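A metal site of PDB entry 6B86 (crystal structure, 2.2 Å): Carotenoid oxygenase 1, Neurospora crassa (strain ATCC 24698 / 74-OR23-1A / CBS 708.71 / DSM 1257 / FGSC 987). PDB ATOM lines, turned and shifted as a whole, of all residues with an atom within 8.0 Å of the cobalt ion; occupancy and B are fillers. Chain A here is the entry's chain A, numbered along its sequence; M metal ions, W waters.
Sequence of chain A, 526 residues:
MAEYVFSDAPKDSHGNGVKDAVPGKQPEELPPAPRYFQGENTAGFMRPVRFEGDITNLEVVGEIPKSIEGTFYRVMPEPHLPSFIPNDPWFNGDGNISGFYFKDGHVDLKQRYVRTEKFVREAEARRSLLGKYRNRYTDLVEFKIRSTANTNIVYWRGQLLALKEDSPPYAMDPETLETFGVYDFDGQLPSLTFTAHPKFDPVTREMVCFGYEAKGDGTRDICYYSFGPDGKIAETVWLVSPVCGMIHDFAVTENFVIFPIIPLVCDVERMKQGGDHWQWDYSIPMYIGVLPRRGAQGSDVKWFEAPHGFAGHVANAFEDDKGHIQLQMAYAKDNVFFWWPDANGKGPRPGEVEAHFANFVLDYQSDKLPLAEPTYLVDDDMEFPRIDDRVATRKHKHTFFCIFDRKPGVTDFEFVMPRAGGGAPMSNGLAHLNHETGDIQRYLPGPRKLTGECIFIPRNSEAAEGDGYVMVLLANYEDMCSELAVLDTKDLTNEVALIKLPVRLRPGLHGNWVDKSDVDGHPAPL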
ATOM      1  N   PHE A  91      -5.557 -17.178   1.839  1.00  0.00           N
ATOM      2  CA  PHE A  91      -5.326 -18.552   1.301  1.00  0.00           C
ATOM      3  C   PHE A  91      -5.457 -19.711   2.299  1.00  0.00           C
ATOM      4  O   PHE A  91      -5.475 -20.875   1.858  1.00  0.00           O
ATOM      5  CB  PHE A  91      -3.928 -18.683   0.655  1.00  0.00           C
ATOM      6  CG  PHE A  91      -3.758 -17.977  -0.672  1.00  0.00           C
ATOM      7  CD1 PHE A  91      -4.838 -17.330  -1.319  1.00  0.00           C
ATOM      8  CD2 PHE A  91      -2.502 -17.944  -1.284  1.00  0.00           C
ATOM      9  CE1 PHE A  91      -4.659 -16.675  -2.526  1.00  0.00           C
ATOM     10  CE2 PHE A  91      -2.329 -17.313  -2.508  1.00  0.00           C
ATOM     11  CZ  PHE A  91      -3.402 -16.688  -3.127  1.00  0.00           C
ATOM     12  N   THR A 151      -9.517 -23.662  -3.161  1.00  0.00           N
ATOM     13  CA  THR A 151      -8.931 -22.957  -4.308  1.00  0.00           C
ATOM     14  C   THR A 151      -9.746 -23.073  -5.584  1.00  0.00           C
ATOM     15  O   THR A 151      -9.926 -22.090  -6.274  1.00  0.00           O
ATOM     16  CB  THR A 151      -7.472 -23.427  -4.555  1.00  0.00           C
ATOM     17  OG1 THR A 151      -6.738 -23.306  -3.343  1.00  0.00           O
ATOM     18  CG2 THR A 151      -6.793 -22.579  -5.618  1.00  0.00           C
ATOM     19  N   ASN A 152     -10.190 -24.276  -5.920  1.00  0.00           N
ATOM     20  CA  ASN A 152     -11.002 -24.487  -7.117  1.00  0.00           C
ATOM     21  C   ASN A 152     -12.003 -25.625  -6.866  1.00  0.00           C
ATOM     22  O   ASN A 152     -11.816 -26.438  -5.958  1.00  0.00           O
ATOM     23  CB  ASN A 152     -10.120 -24.801  -8.336  1.00  0.00           C
ATOM     24  CG  ASN A 152     -10.820 -24.560  -9.662  1.00  0.00           C
ATOM     25  OD1 ASN A 152     -11.990 -24.186  -9.719  1.00  0.00           O
ATOM     26  ND2 ASN A 152     -10.098 -24.769 -10.758  1.00  0.00           N
ATOM     27  N   GLU A 165      -3.697 -27.234  -3.665  1.00  0.00           N
ATOM     28  CA  GLU A 165      -2.472 -27.726  -4.307  1.00  0.00           C
ATOM     29  C   GLU A 165      -1.466 -28.451  -3.383  1.00  0.00           C
ATOM     30  O   GLU A 165      -0.503 -29.037  -3.884  1.00  0.00           O
ATOM     31  CB  GLU A 165      -1.773 -26.574  -5.063  1.00  0.00           C
ATOM     32  CG  GLU A 165      -1.102 -25.514  -4.191  1.00  0.00           C
ATOM     33  CD  GLU A 165      -0.912 -24.202  -4.896  1.00  0.00           C
ATOM     34  OE1 GLU A 165       0.210 -23.646  -4.750  1.00  0.00           O
ATOM     35  OE2 GLU A 165      -1.850 -23.718  -5.578  1.00  0.00           O
ATOM     36  N   THR A 195      -2.961 -30.476  -8.293  1.00  0.00           N
ATOM     37  CA  THR A 195      -3.081 -29.056  -8.650  1.00  0.00           C
ATOM     38  C   THR A 195      -4.528 -28.539  -8.578  1.00  0.00           C
ATOM     39  O   THR A 195      -5.485 -29.275  -8.833  1.00  0.00           O
ATOM     40  CB  THR A 195      -2.554 -28.784 -10.083  1.00  0.00           C
ATOM     41  OG1 THR A 195      -2.638 -27.378 -10.381  1.00  0.00           O
ATOM     42  CG2 THR A 195      -3.359 -29.526 -11.140  1.00  0.00           C
ATOM     43  N   ALA A 196      -4.663 -27.264  -8.272  1.00  0.00           N
ATOM     44  CA  ALA A 196      -5.943 -26.575  -8.342  1.00  0.00           C
ATOM     45  C   ALA A 196      -6.369 -26.216  -9.756  1.00  0.00           C
ATOM     46  O   ALA A 196      -7.486 -25.736  -9.964  1.00  0.00           O
ATOM     47  CB  ALA A 196      -5.902 -25.326  -7.483  1.00  0.00           C
ATOM     48  N   HIS A 197      -5.489 -26.434 -10.740  1.00  0.00           N
ATOM     49  CA  HIS A 197      -5.773 -26.040 -12.115  1.00  0.00           C
ATOM     50  C   HIS A 197      -5.532 -27.164 -13.110  1.00  0.00           C
ATOM     51  O   HIS A 197      -4.744 -27.020 -14.039  1.00  0.00           O
ATOM     52  CB  HIS A 197      -4.918 -24.822 -12.461  1.00  0.00           C
ATOM     53  CG  HIS A 197      -5.355 -23.584 -11.745  1.00  0.00           C
ATOM     54  ND1 HIS A 197      -6.514 -22.936 -12.084  1.00  0.00           N
ATOM     55  CD2 HIS A 197      -4.822 -22.898 -10.704  1.00  0.00           C
ATOM     56  CE1 HIS A 197      -6.683 -21.906 -11.282  1.00  0.00           C
ATOM     57  NE2 HIS A 197      -5.670 -21.852 -10.430  1.00  0.00           N
ATOM     58  N   HIS A 248       1.707 -23.011  -9.377  1.00  0.00           N
ATOM     59  CA  HIS A 248       0.269 -22.859  -9.133  1.00  0.00           C
ATOM     60  C   HIS A 248      -0.600 -23.313 -10.303  1.00  0.00           C
ATOM     61  O   HIS A 248      -1.634 -23.945 -10.096  1.00  0.00           O
ATOM     62  CB  HIS A 248      -0.082 -21.417  -8.804  1.00  0.00           C
ATOM     63  CG  HIS A 248      -1.523 -21.218  -8.483  1.00  0.00           C
ATOM     64  ND1 HIS A 248      -2.121 -21.781  -7.373  1.00  0.00           N
ATOM     65  CD2 HIS A 248      -2.503 -20.533  -9.131  1.00  0.00           C
ATOM     66  CE1 HIS A 248      -3.400 -21.440  -7.345  1.00  0.00           C
ATOM     67  NE2 HIS A 248      -3.659 -20.681  -8.396  1.00  0.00           N
ATOM     68  N   ASP A 249      -0.193 -22.943 -11.513  1.00  0.00           N
ATOM     69  CA  ASP A 249      -0.964 -23.215 -12.711  1.00  0.00           C
ATOM     70  C   ASP A 249      -0.043 -23.886 -13.710  1.00  0.00           C
ATOM     71  O   ASP A 249       1.165 -23.947 -13.489  1.00  0.00           O
ATOM     72  CB  ASP A 249      -1.524 -21.894 -13.260  1.00  0.00           C
ATOM     73  CG  ASP A 249      -2.774 -22.068 -14.121  1.00  0.00           C
ATOM     74  OD1 ASP A 249      -3.019 -23.183 -14.634  1.00  0.00           O
ATOM     75  OD2 ASP A 249      -3.494 -21.060 -14.315  1.00  0.00           O
ATOM     76  N   GLY A 312       1.459 -15.703 -13.160  1.00  0.00           N
ATOM     77  CA  GLY A 312       0.024 -15.638 -12.848  1.00  0.00           C
ATOM     78  C   GLY A 312      -0.740 -16.770 -13.534  1.00  0.00           C
ATOM     79  O   GLY A 312      -0.157 -17.733 -14.037  1.00  0.00           O
ATOM     80  N   HIS A 313      -2.062 -16.628 -13.580  1.00  0.00           N
ATOM     81  CA  HIS A 313      -2.899 -17.690 -14.144  1.00  0.00           C
ATOM     82  C   HIS A 313      -2.746 -17.826 -15.660  1.00  0.00           C
ATOM     83  O   HIS A 313      -2.630 -16.829 -16.374  1.00  0.00           O
ATOM     84  CB  HIS A 313      -4.360 -17.488 -13.767  1.00  0.00           C
ATOM     85  CG  HIS A 313      -4.647 -17.799 -12.334  1.00  0.00           C
ATOM     86  ND1 HIS A 313      -4.823 -16.822 -11.369  1.00  0.00           N
ATOM     87  CD2 HIS A 313      -4.754 -18.983 -11.696  1.00  0.00           C
ATOM     88  CE1 HIS A 313      -5.068 -17.400 -10.209  1.00  0.00           C
ATOM     89  NE2 HIS A 313      -5.028 -18.713 -10.375  1.00  0.00           N
ATOM     90  N   VAL A 314      -2.758 -19.053 -16.138  1.00  0.00           N
ATOM     91  CA  VAL A 314      -2.761 -19.345 -17.555  1.00  0.00           C
ATOM     92  C   VAL A 314      -4.162 -19.126 -18.136  1.00  0.00           C
ATOM     93  O   VAL A 314      -5.154 -19.615 -17.600  1.00  0.00           O
ATOM     94  CB  VAL A 314      -2.337 -20.795 -17.812  1.00  0.00           C
ATOM     95  CG1 VAL A 314      -2.468 -21.170 -19.276  1.00  0.00           C
ATOM     96  CG2 VAL A 314      -0.916 -21.009 -17.297  1.00  0.00           C
ATOM     97  N   PHE A 337       2.548 -12.017  -4.347  1.00  0.00           N
ATOM     98  CA  PHE A 337       2.313 -12.456  -2.964  1.00  0.00           C
ATOM     99  C   PHE A 337       3.325 -11.797  -1.990  1.00  0.00           C
ATOM    100  O   PHE A 337       4.182 -12.450  -1.376  1.00  0.00           O
ATOM    101  CB  PHE A 337       2.332 -14.001  -2.870  1.00  0.00           C
ATOM    102  CG  PHE A 337       1.334 -14.728  -3.771  1.00  0.00           C
ATOM    103  CD1 PHE A 337       0.238 -14.090  -4.364  1.00  0.00           C
ATOM    104  CD2 PHE A 337       1.497 -16.102  -4.020  1.00  0.00           C
ATOM    105  CE1 PHE A 337      -0.645 -14.794  -5.199  1.00  0.00           C
ATOM    106  CE2 PHE A 337       0.612 -16.802  -4.826  1.00  0.00           C
ATOM    107  CZ  PHE A 337      -0.461 -16.155  -5.421  1.00  0.00           C
ATOM    108  N   GLU A 383      -6.047 -10.165 -14.271  1.00  0.00           N
ATOM    109  CA  GLU A 383      -5.890 -11.537 -13.749  1.00  0.00           C
ATOM    110  C   GLU A 383      -7.190 -12.334 -14.004  1.00  0.00           C
ATOM    111  O   GLU A 383      -8.137 -11.828 -14.625  1.00  0.00           O
ATOM    112  CB  GLU A 383      -5.499 -11.530 -12.235  1.00  0.00           C
ATOM    113  CG  GLU A 383      -4.089 -12.045 -11.911  1.00  0.00           C
ATOM    114  CD  GLU A 383      -3.862 -13.554 -12.172  1.00  0.00           C
ATOM    115  OE1 GLU A 383      -2.700 -14.042 -12.145  1.00  0.00           O
ATOM    116  OE2 GLU A 383      -4.855 -14.268 -12.392  1.00  0.00           O
ATOM    117  N   PHE A 384      -7.201 -13.584 -13.538  1.00  0.00           N
ATOM    118  CA  PHE A 384      -8.355 -14.474 -13.628  1.00  0.00           C
ATOM    119  C   PHE A 384      -8.899 -14.622 -15.048  1.00  0.00           C
ATOM    120  O   PHE A 384     -10.080 -14.404 -15.304  1.00  0.00           O
ATOM    121  CB  PHE A 384      -9.427 -14.044 -12.607  1.00  0.00           C
ATOM    122  CG  PHE A 384      -8.989 -14.202 -11.179  1.00  0.00           C
ATOM    123  CD1 PHE A 384      -8.864 -15.469 -10.598  1.00  0.00           C
ATOM    124  CD2 PHE A 384      -8.642 -13.081 -10.412  1.00  0.00           C
ATOM    125  CE1 PHE A 384      -8.412 -15.613  -9.299  1.00  0.00           C
ATOM    126  CE2 PHE A 384      -8.202 -13.223  -9.094  1.00  0.00           C
ATOM    127  CZ  PHE A 384      -8.088 -14.493  -8.541  1.00  0.00           C
ATOM    128  N   GLU A 453     -13.843 -13.806 -10.109  1.00  0.00           N
ATOM    129  CA  GLU A 453     -13.576 -14.484 -11.385  1.00  0.00           C
ATOM    130  C   GLU A 453     -14.891 -14.791 -12.088  1.00  0.00           C
ATOM    131  O   GLU A 453     -15.847 -15.265 -11.463  1.00  0.00           O
ATOM    132  CB  GLU A 453     -12.823 -15.791 -11.172  1.00  0.00           C
ATOM    133  CG  GLU A 453     -12.485 -16.571 -12.436  1.00  0.00           C
ATOM    134  CD  GLU A 453     -12.047 -18.009 -12.152  1.00  0.00           C
ATOM    135  OE1 GLU A 453     -12.880 -18.784 -11.644  1.00  0.00           O
ATOM    136  OE2 GLU A 453     -10.892 -18.369 -12.478  1.00  0.00           O
ATOM    137  N   LEU A 509     -12.120 -17.551  -4.763  1.00  0.00           N
ATOM    138  CA  LEU A 509     -11.157 -17.919  -5.762  1.00  0.00           C
ATOM    139  C   LEU A 509     -11.905 -18.438  -6.974  1.00  0.00           C
ATOM    140  O   LEU A 509     -12.721 -17.705  -7.540  1.00  0.00           O
ATOM    141  CB  LEU A 509     -10.134 -18.896  -5.143  1.00  0.00           C
ATOM    142  CG  LEU A 509      -9.144 -18.213  -4.194  1.00  0.00           C
ATOM    143  CD1 LEU A 509      -8.452 -19.186  -3.267  1.00  0.00           C
ATOM    144  CD2 LEU A 509      -8.082 -17.459  -5.004  1.00  0.00           C
ATOM    145  N   HIS A 510     -11.657 -19.678  -7.389  1.00  0.00           N
ATOM    146  CA  HIS A 510     -12.089 -20.116  -8.708  1.00  0.00           C
ATOM    147  C   HIS A 510     -13.487 -20.727  -8.695  1.00  0.00           C
ATOM    148  O   HIS A 510     -14.010 -21.120  -7.656  1.00  0.00           O
ATOM    149  CB  HIS A 510     -11.058 -21.093  -9.303  1.00  0.00           C
ATOM    150  CG  HIS A 510      -9.718 -20.469  -9.489  1.00  0.00           C
ATOM    151  ND1 HIS A 510      -9.449 -19.567 -10.493  1.00  0.00           N
ATOM    152  CD2 HIS A 510      -8.576 -20.568  -8.769  1.00  0.00           C
ATOM    153  CE1 HIS A 510      -8.203 -19.151 -10.390  1.00  0.00           C
ATOM    154  NE2 HIS A 510      -7.650 -19.746  -9.343  1.00  0.00           N
HETATM  155 CO    CO M   1      -5.586 -20.221  -9.191  1.00  0.00          CO
HETATM  156  O   HOH W   1      -5.758 -19.437  -7.326  1.00  0.00           O
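Of the 18 residues printed, 4 come within 4 Å of the cobalt ion. The nearest printed residue that does not touch the cobalt ion is Thr 151 (4.4 Å).
A ring nitrogen (ND1) of His 313 sits at hydrogen-bond distance from the side-chain carboxylate (OE2) of Glu 383 (2.8 Å). The backbone NH of His 197 is in hydrogen-bond range of the side-chain hydroxyl of Thr 195, at 3.0 Å. The backbone NH of His 510 is in hydrogen-bond range of the backbone carbonyl oxygen of Thr 151 (3.2 Å). The side-chain carboxylate (OE2) of Glu 453 sits at hydrogen-bond distance from a ring nitrogen (ND1) of His 510 (2.7 Å). A ring nitrogen (ND1) of His 248 sits at hydrogen-bond distance from the side-chain carboxylate (OE2) of Glu 165, at 2.7 Å.
The cobalt ion is bound by NE2 of His 313 (2.0 Å), water W1 (2.0 Å), NE2 of His 197 (2.0 Å), NE2 of His 510 (2.1 Å) and NE2 of His 248 (2.1 Å). The cobalt ion has five donor atoms within binding distance.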
